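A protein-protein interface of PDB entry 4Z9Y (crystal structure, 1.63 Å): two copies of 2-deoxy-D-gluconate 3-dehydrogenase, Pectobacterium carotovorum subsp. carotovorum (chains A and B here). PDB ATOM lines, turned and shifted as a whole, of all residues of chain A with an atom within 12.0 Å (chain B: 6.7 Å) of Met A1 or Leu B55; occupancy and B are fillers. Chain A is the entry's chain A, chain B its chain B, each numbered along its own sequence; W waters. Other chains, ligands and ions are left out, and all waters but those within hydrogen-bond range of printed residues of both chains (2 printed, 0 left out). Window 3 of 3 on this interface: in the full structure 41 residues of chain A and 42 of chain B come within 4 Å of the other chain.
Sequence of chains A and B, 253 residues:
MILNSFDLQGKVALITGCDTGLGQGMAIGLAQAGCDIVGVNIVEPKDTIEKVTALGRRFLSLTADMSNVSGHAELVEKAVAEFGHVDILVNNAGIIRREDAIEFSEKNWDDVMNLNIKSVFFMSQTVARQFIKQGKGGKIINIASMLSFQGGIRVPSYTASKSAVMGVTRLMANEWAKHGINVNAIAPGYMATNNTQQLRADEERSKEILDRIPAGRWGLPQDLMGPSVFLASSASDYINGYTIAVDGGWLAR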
ATOM      1  N   MET A   1      14.122  -7.894 -24.330  1.00  0.00           N
ATOM      2  CA  MET A   1      14.358  -6.464 -23.993  1.00  0.00           C
ATOM      3  C   MET A   1      15.806  -6.258 -23.552  1.00  0.00           C
ATOM      4  O   MET A   1      16.251  -6.820 -22.545  1.00  0.00           O
ATOM      5  CB  MET A   1      13.386  -6.004 -22.899  1.00  0.00           C
ATOM      6  CG  MET A   1      11.926  -6.012 -23.329  1.00  0.00           C
ATOM      7  SD  MET A   1      11.550  -4.732 -24.550  1.00  0.00           S
ATOM      8  CE  MET A   1      11.690  -3.243 -23.577  1.00  0.00           C
ATOM      9  N   ILE A   2      16.527  -5.419 -24.293  1.00  0.00           N
ATOM     10  CA  ILE A   2      17.983  -5.370 -24.190  1.00  0.00           C
ATOM     11  C   ILE A   2      18.533  -5.058 -22.797  1.00  0.00           C
ATOM     12  O   ILE A   2      19.609  -5.533 -22.456  1.00  0.00           O
ATOM     13  CB  ILE A   2      18.587  -4.382 -25.212  1.00  0.00           C
ATOM     14  CG1 ILE A   2      20.094  -4.640 -25.377  1.00  0.00           C
ATOM     15  CG2 ILE A   2      18.311  -2.938 -24.808  1.00  0.00           C
ATOM     16  CD1 ILE A   2      20.440  -6.064 -25.769  1.00  0.00           C
ATOM     17  N   LEU A   3      17.831  -4.261 -21.996  1.00  0.00           N
ATOM     18  CA  LEU A   3      18.374  -3.929 -20.681  1.00  0.00           C
ATOM     19  C   LEU A   3      18.519  -5.201 -19.831  1.00  0.00           C
ATOM     20  O   LEU A   3      19.407  -5.263 -18.976  1.00  0.00           O
ATOM     21  CB  LEU A   3      17.577  -2.842 -19.960  1.00  0.00           C
ATOM     22  CG  LEU A   3      17.626  -1.484 -20.682  1.00  0.00           C
ATOM     23  CD1 LEU A   3      16.666  -0.475 -20.076  1.00  0.00           C
ATOM     24  CD2 LEU A   3      19.044  -0.913 -20.727  1.00  0.00           C
ATOM     25  N   ASN A   4      17.683  -6.215 -20.077  1.00  0.00           N
ATOM     26  CA  ASN A   4      17.800  -7.475 -19.342  1.00  0.00           C
ATOM     27  C   ASN A   4      19.133  -8.180 -19.626  1.00  0.00           C
ATOM     28  O   ASN A   4      19.637  -8.922 -18.770  1.00  0.00           O
ATOM     29  CB  ASN A   4      16.626  -8.416 -19.654  1.00  0.00           C
ATOM     30  CG  ASN A   4      15.285  -7.880 -19.162  1.00  0.00           C
ATOM     31  OD1 ASN A   4      14.231  -8.184 -19.737  1.00  0.00           O
ATOM     32  ND2 ASN A   4      15.309  -7.095 -18.103  1.00  0.00           N
ATOM     33  N   SER A   5      19.714  -7.932 -20.799  1.00  0.00           N
ATOM     34  CA  SER A   5      20.992  -8.543 -21.185  1.00  0.00           C
ATOM     35  C   SER A   5      22.174  -8.095 -20.328  1.00  0.00           C
ATOM     36  O   SER A   5      23.181  -8.797 -20.262  1.00  0.00           O
ATOM     37  CB  SER A   5      21.316  -8.248 -22.647  1.00  0.00           C
ATOM     38  OG  SER A   5      20.362  -8.849 -23.483  1.00  0.00           O
ATOM     39  N   PHE A   6      22.062  -6.939 -19.686  1.00  0.00           N
ATOM     40  CA  PHE A   6      23.137  -6.431 -18.831  1.00  0.00           C
ATOM     41  C   PHE A   6      23.010  -6.919 -17.398  1.00  0.00           C
ATOM     42  O   PHE A   6      23.935  -6.763 -16.604  1.00  0.00           O
ATOM     43  CB  PHE A   6      23.121  -4.901 -18.791  1.00  0.00           C
ATOM     44  CG  PHE A   6      23.317  -4.250 -20.126  1.00  0.00           C
ATOM     45  CD1 PHE A   6      24.566  -4.181 -20.713  1.00  0.00           C
ATOM     46  CD2 PHE A   6      22.252  -3.661 -20.780  1.00  0.00           C
ATOM     47  CE1 PHE A   6      24.738  -3.558 -21.949  1.00  0.00           C
ATOM     48  CE2 PHE A   6      22.422  -3.049 -22.016  1.00  0.00           C
ATOM     49  CZ  PHE A   6      23.661  -3.003 -22.602  1.00  0.00           C
ATOM     50  N   ASP A   7      21.843  -7.462 -17.057  1.00  0.00           N
ATOM     51  CA  ASP A   7      21.521  -7.852 -15.690  1.00  0.00           C
ATOM     52  C   ASP A   7      22.245  -9.141 -15.334  1.00  0.00           C
ATOM     53  O   ASP A   7      22.085 -10.163 -16.006  1.00  0.00           O
ATOM     54  CB  ASP A   7      20.006  -8.033 -15.571  1.00  0.00           C
ATOM     55  CG  ASP A   7      19.529  -8.206 -14.153  1.00  0.00           C
ATOM     56  OD1 ASP A   7      20.317  -8.541 -13.248  1.00  0.00           O
ATOM     57  OD2 ASP A   7      18.309  -8.030 -13.953  1.00  0.00           O
ATOM     58  N   LEU A   8      23.036  -9.091 -14.266  1.00  0.00           N
ATOM     59  CA  LEU A   8      23.845 -10.223 -13.849  1.00  0.00           C
ATOM     60  C   LEU A   8      23.282 -10.905 -12.606  1.00  0.00           C
ATOM     61  O   LEU A   8      24.011 -11.590 -11.892  1.00  0.00           O
ATOM     62  CB  LEU A   8      25.298  -9.786 -13.609  1.00  0.00           C
ATOM     63  CG  LEU A   8      25.996  -9.148 -14.823  1.00  0.00           C
ATOM     64  CD1 LEU A   8      27.431  -8.779 -14.500  1.00  0.00           C
ATOM     65  CD2 LEU A   8      25.954 -10.059 -16.037  1.00  0.00           C
ATOM     66  N   GLN A   9      21.980 -10.756 -12.364  1.00  0.00           N
ATOM     67  CA  GLN A   9      21.365 -11.449 -11.246  1.00  0.00           C
ATOM     68  C   GLN A   9      21.647 -12.942 -11.364  1.00  0.00           C
ATOM     69  O   GLN A   9      21.582 -13.511 -12.446  1.00  0.00           O
ATOM     70  CB  GLN A   9      19.846 -11.204 -11.208  1.00  0.00           C
ATOM     71  CG  GLN A   9      19.084 -11.692 -12.438  1.00  0.00           C
ATOM     72  CD  GLN A   9      17.565 -11.662 -12.267  1.00  0.00           C
ATOM     73  OE1 GLN A   9      17.039 -11.888 -11.171  1.00  0.00           O
ATOM     74  NE2 GLN A   9      16.852 -11.396 -13.363  1.00  0.00           N
ATOM     75  N   SER A 233      28.481  -9.804 -19.441  1.00  0.00           N
ATOM     76  CA  SER A 233      27.045 -10.000 -19.677  1.00  0.00           C
ATOM     77  C   SER A 233      26.732 -10.529 -21.071  1.00  0.00           C
ATOM     78  O   SER A 233      27.576 -10.509 -21.970  1.00  0.00           O
ATOM     79  CB  SER A 233      26.296  -8.687 -19.467  1.00  0.00           C
ATOM     80  OG  SER A 233      26.412  -7.845 -20.600  1.00  0.00           O
ATOM     81  N   SER A 234      25.488 -10.968 -21.253  1.00  0.00           N
ATOM     82  CA  SER A 234      25.039 -11.448 -22.556  1.00  0.00           C
ATOM     83  C   SER A 234      24.958 -10.324 -23.584  1.00  0.00           C
ATOM     84  O   SER A 234      24.822 -10.606 -24.768  1.00  0.00           O
ATOM     85  CB  SER A 234      23.688 -12.163 -22.459  1.00  0.00           C
ATOM     86  OG  SER A 234      22.669 -11.283 -22.063  1.00  0.00           O
ATOM     87  N   ALA A 235      25.044  -9.080 -23.132  1.00  0.00           N
ATOM     88  CA  ALA A 235      25.018  -7.922 -24.039  1.00  0.00           C
ATOM     89  C   ALA A 235      26.251  -7.855 -24.937  1.00  0.00           C
ATOM     90  O   ALA A 235      26.274  -7.085 -25.901  1.00  0.00           O
ATOM     91  CB  ALA A 235      24.874  -6.627 -23.245  1.00  0.00           C
ATOM     92  N   SER A 236      27.286  -8.637 -24.629  1.00  0.00           N
ATOM     93  CA  SER A 236      28.514  -8.632 -25.418  1.00  0.00           C
ATOM     94  C   SER A 236      28.847 -10.006 -25.992  1.00  0.00           C
ATOM     95  O   SER A 236      30.011 -10.313 -26.240  1.00  0.00           O
ATOM     96  CB  SER A 236      29.683  -8.120 -24.572  1.00  0.00           C
ATOM     97  OG  SER A 236      29.894  -8.930 -23.436  1.00  0.00           O
ATOM     98  N   ASP A 237      27.824 -10.828 -26.225  1.00  0.00           N
ATOM     99  CA  ASP A 237      28.045 -12.219 -26.632  1.00  0.00           C
ATOM    100  C   ASP A 237      28.835 -12.428 -27.926  1.00  0.00           C
ATOM    101  O   ASP A 237      29.494 -13.449 -28.059  1.00  0.00           O
ATOM    102  CB  ASP A 237      26.701 -12.969 -26.724  1.00  0.00           C
ATOM    103  CG  ASP A 237      26.204 -13.467 -25.371  1.00  0.00           C
ATOM    104  OD1 ASP A 237      26.951 -13.409 -24.365  1.00  0.00           O
ATOM    105  OD2 ASP A 237      25.049 -13.970 -25.316  1.00  0.00           O
ATOM    106  N   ALA B  27      18.603   0.444 -33.997  1.00  0.00           N
ATOM    107  CA  ALA B  27      17.484   1.304 -33.655  1.00  0.00           C
ATOM    108  C   ALA B  27      16.543   0.644 -32.652  1.00  0.00           C
ATOM    109  O   ALA B  27      16.087   1.277 -31.705  1.00  0.00           O
ATOM    110  CB  ALA B  27      16.708   1.713 -34.902  1.00  0.00           C
ATOM    111  N   ILE B  28      16.250  -0.637 -32.875  1.00  0.00           N
ATOM    112  CA  ILE B  28      15.353  -1.374 -31.993  1.00  0.00           C
ATOM    113  C   ILE B  28      15.983  -1.532 -30.610  1.00  0.00           C
ATOM    114  O   ILE B  28      15.311  -1.321 -29.600  1.00  0.00           O
ATOM    115  CB  ILE B  28      14.937  -2.731 -32.588  1.00  0.00           C
ATOM    116  CG1 ILE B  28      14.050  -2.488 -33.811  1.00  0.00           C
ATOM    117  CG2 ILE B  28      14.155  -3.541 -31.576  1.00  0.00           C
ATOM    118  CD1 ILE B  28      13.894  -3.700 -34.706  1.00  0.00           C
ATOM    119  N   GLY B  29      17.272  -1.865 -30.579  1.00  0.00           N
ATOM    120  CA  GLY B  29      17.999  -1.996 -29.316  1.00  0.00           C
ATOM    121  C   GLY B  29      17.972  -0.714 -28.504  1.00  0.00           C
ATOM    122  O   GLY B  29      17.648  -0.707 -27.308  1.00  0.00           O
ATOM    123  N   LEU B  30      18.291   0.395 -29.163  1.00  0.00           N
ATOM    124  CA  LEU B  30      18.256   1.692 -28.520  1.00  0.00           C
ATOM    125  C   LEU B  30      16.856   2.034 -28.000  1.00  0.00           C
ATOM    126  O   LEU B  30      16.706   2.569 -26.883  1.00  0.00           O
ATOM    127  CB  LEU B  30      18.805   2.769 -29.459  1.00  0.00           C
ATOM    128  CG  LEU B  30      20.315   2.665 -29.691  1.00  0.00           C
ATOM    129  CD1 LEU B  30      20.731   3.432 -30.932  1.00  0.00           C
ATOM    130  CD2 LEU B  30      21.111   3.120 -28.482  1.00  0.00           C
ATOM    131  N   ALA B  31      15.830   1.708 -28.791  1.00  0.00           N
ATOM    132  CA  ALA B  31      14.445   1.922 -28.369  1.00  0.00           C
ATOM    133  C   ALA B  31      14.067   1.061 -27.161  1.00  0.00           C
ATOM    134  O   ALA B  31      13.403   1.533 -26.225  1.00  0.00           O
ATOM    135  CB  ALA B  31      13.491   1.680 -29.537  1.00  0.00           C
ATOM    136  N   GLN B  32      14.521  -0.184 -27.169  1.00  0.00           N
ATOM    137  CA  GLN B  32      14.296  -1.098 -26.047  1.00  0.00           C
ATOM    138  C   GLN B  32      14.912  -0.561 -24.748  1.00  0.00           C
ATOM    139  O   GLN B  32      14.361  -0.742 -23.658  1.00  0.00           O
ATOM    140  CB  GLN B  32      14.853  -2.477 -26.360  1.00  0.00           C
ATOM    141  CG  GLN B  32      14.033  -3.284 -27.362  1.00  0.00           C
ATOM    142  CD  GLN B  32      14.570  -4.683 -27.548  1.00  0.00           C
ATOM    143  OE1 GLN B  32      15.529  -5.089 -26.887  1.00  0.00           O
ATOM    144  NE2 GLN B  32      13.954  -5.437 -28.462  1.00  0.00           N
ATOM    145  N   ALA B  33      16.048   0.114 -24.878  1.00  0.00           N
ATOM    146  CA  ALA B  33      16.730   0.730 -23.740  1.00  0.00           C
ATOM    147  C   ALA B  33      16.105   2.045 -23.287  1.00  0.00           C
ATOM    148  O   ALA B  33      16.523   2.593 -22.275  1.00  0.00           O
ATOM    149  CB  ALA B  33      18.206   0.934 -24.063  1.00  0.00           C
ATOM    150  N   GLU B  50       7.236   0.133 -36.890  1.00  0.00           N
ATOM    151  CA  GLU B  50       6.278  -0.730 -36.210  1.00  0.00           C
ATOM    152  C   GLU B  50       6.860  -1.258 -34.905  1.00  0.00           C
ATOM    153  O   GLU B  50       6.227  -1.178 -33.867  1.00  0.00           O
ATOM    154  CB  GLU B  50       5.855  -1.900 -37.103  1.00  0.00           C
ATOM    155  CG  GLU B  50       5.016  -1.486 -38.305  1.00  0.00           C
ATOM    156  CD  GLU B  50       4.567  -2.659 -39.159  1.00  0.00           C
ATOM    157  OE1 GLU B  50       4.805  -3.829 -38.762  1.00  0.00           O
ATOM    158  OE2 GLU B  50       3.959  -2.407 -40.233  1.00  0.00           O
ATOM    159  N   LYS B  51       8.088  -1.758 -34.969  1.00  0.00           N
ATOM    160  CA  LYS B  51       8.711  -2.377 -33.804  1.00  0.00           C
ATOM    161  C   LYS B  51       9.035  -1.358 -32.717  1.00  0.00           C
ATOM    162  O   LYS B  51       8.801  -1.600 -31.530  1.00  0.00           O
ATOM    163  CB  LYS B  51       9.948  -3.172 -34.237  1.00  0.00           C
ATOM    164  CG  LYS B  51       9.577  -4.447 -34.984  1.00  0.00           C
ATOM    165  CD  LYS B  51      10.713  -5.035 -35.798  1.00  0.00           C
ATOM    166  CE  LYS B  51      10.290  -6.363 -36.422  1.00  0.00           C
ATOM    167  NZ  LYS B  51      11.311  -6.944 -37.335  1.00  0.00           N
ATOM    168  N   VAL B  52       9.552  -0.203 -33.122  1.00  0.00           N
ATOM    169  CA  VAL B  52       9.865   0.855 -32.177  1.00  0.00           C
ATOM    170  C   VAL B  52       8.605   1.380 -31.480  1.00  0.00           C
ATOM    171  O   VAL B  52       8.588   1.553 -30.268  1.00  0.00           O
ATOM    172  CB  VAL B  52      10.651   2.002 -32.859  1.00  0.00           C
ATOM    173  CG1 VAL B  52      10.728   3.235 -31.969  1.00  0.00           C
ATOM    174  CG2 VAL B  52      12.046   1.518 -33.225  1.00  0.00           C
ATOM    175  N   THR B  53       7.544   1.620 -32.241  1.00  0.00           N
ATOM    176  CA  THR B  53       6.323   2.167 -31.657  1.00  0.00           C
ATOM    177  C   THR B  53       5.579   1.128 -30.811  1.00  0.00           C
ATOM    178  O   THR B  53       4.877   1.474 -29.854  1.00  0.00           O
ATOM    179  CB  THR B  53       5.402   2.780 -32.732  1.00  0.00           C
ATOM    180  OG1 THR B  53       5.100   1.799 -33.719  1.00  0.00           O
ATOM    181  CG2 THR B  53       6.092   3.933 -33.397  1.00  0.00           C
ATOM    182  N   ALA B  54       5.778  -0.148 -31.133  1.00  0.00           N
ATOM    183  CA  ALA B  54       5.240  -1.235 -30.320  1.00  0.00           C
ATOM    184  C   ALA B  54       5.823  -1.238 -28.907  1.00  0.00           C
ATOM    185  O   ALA B  54       5.172  -1.679 -27.970  1.00  0.00           O
ATOM    186  CB  ALA B  54       5.480  -2.577 -30.979  1.00  0.00           C
ATOM    187  N   LEU B  55       7.041  -0.722 -28.762  1.00  0.00           N
ATOM    188  CA  LEU B  55       7.677  -0.576 -27.444  1.00  0.00           C
ATOM    189  C   LEU B  55       7.164   0.615 -26.645  1.00  0.00           C
ATOM    190  O   LEU B  55       7.575   0.818 -25.496  1.00  0.00           O
ATOM    191  CB  LEU B  55       9.194  -0.429 -27.628  1.00  0.00           C
ATOM    192  CG  LEU B  55       9.886  -1.644 -28.239  1.00  0.00           C
ATOM    193  CD1 LEU B  55      11.266  -1.282 -28.752  1.00  0.00           C
ATOM    194  CD2 LEU B  55       9.979  -2.760 -27.207  1.00  0.00           C
ATOM    195  N   GLY B  56       6.299   1.423 -27.255  1.00  0.00           N
ATOM    196  CA  GLY B  56       5.798   2.634 -26.641  1.00  0.00           C
ATOM    197  C   GLY B  56       6.703   3.830 -26.854  1.00  0.00           C
ATOM    198  O   GLY B  56       6.505   4.878 -26.235  1.00  0.00           O
ATOM    199  N   ARG B  57       7.687   3.683 -27.734  1.00  0.00           N
ATOM    200  CA  ARG B  57       8.622   4.758 -28.051  1.00  0.00           C
ATOM    201  C   ARG B  57       8.185   5.523 -29.298  1.00  0.00           C
ATOM    202  O   ARG B  57       7.387   5.034 -30.100  1.00  0.00           O
ATOM    203  CB  ARG B  57      10.034   4.195 -28.265  1.00  0.00           C
ATOM    204  CG  ARG B  57      10.600   3.437 -27.072  1.00  0.00           C
ATOM    205  CD  ARG B  57      11.241   4.342 -26.033  1.00  0.00           C
ATOM    206  NE  ARG B  57      10.311   5.228 -25.342  1.00  0.00           N
ATOM    207  CZ  ARG B  57       9.575   4.907 -24.279  1.00  0.00           C
ATOM    208  NH1 ARG B  57       9.621   3.693 -23.742  1.00  0.00           N
ATOM    209  NH2 ARG B  57       8.765   5.819 -23.746  1.00  0.00           N
HETATM  210  O   HOH W   1      16.649  -7.632 -26.854  1.00  0.00           O
HETATM  211  O   HOH W   2      15.163  -3.143 -22.339  1.00  0.00           O
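The backbone NH (N) of Ile A2 sits at hydrogen-bond distance from the side-chain amide oxygen (OE1) of Gln B32, 2.8 Å away.
Water W1 bridges OE1 of Gln B32 (2.8 Å) and N of Ile A2 (3.4 Å). Water W2 lies within hydrogen-bond range of the backbone carbonyl oxygen (O) of Gln B32, the backbone NH (N) of Leu A3 and the backbone NH (N) of Ile A2.
Among the printed residues, pairs that only touch across the chains: Met A1 with Gln B32 (3.4 Å), Met A1 with Leu B55 (3.7 Å), Ile A2 with Gly B29 (3.4 Å), Ile A2 with Ala B33 (3.8 Å) and Leu A3 with Ala B33 (3.8 Å).
No position is printed for both chains. Of the 6 pairs that touch across the chains among the printed residues, none has its exchanged pair printed and touching as well.
Of the 15 printed residues of chain B, 4 touch a printed residue of chain A. Printed residues of chain B that touch a printed residue of chain A: Gly B29, Gln B32, Ala B33 and Leu B55. Hydrophobic or aromatic side chains of chain B within 4 Å of the printed part of chain A: Ala B33 and Leu B55. Of the 14 printed residues of chain A, 3 touch a printed residue of chain B. Printed residues of chain A that touch a printed residue of chain B: Met A1, Ile A2 and Leu A3. Among the printed residues, no Asp or Glu carboxylate lies within 4 Å of a Lys or Arg side-chain nitrogen of the other chain.
Of chain A, only Met A1 (3.7 Å) comes within 4 Å of Leu B55. No residue of chain A comes within 4 Å of Ile B28. No residue of chain A comes within 4 Å of Ala B31. Of the printed residues of chain A, Gln B32 touches Met A1 and Ile A2. Printed residues of chain A within 4 Å of Ala B33: Ile A2 and Leu A3. No residue of chain A comes within 4 Å of Val B52. No residue of chain A comes within 4 Å of Thr B53. No residue of chain A comes within 4 Å of Ala B54. No residue of chain A comes within 4 Å of Gly B56. Printed residues of chain B within 4 Å of Leu A3: Ala B33. Printed residues of chain B within 4 Å of Ile A2: Gly B29 (3.4 Å), Gln B32 (2.8 Å) and Ala B33 (3.8 Å). The nearest residue of chain B that does not touch Met A1 is Ala B33 (5.7 Å).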
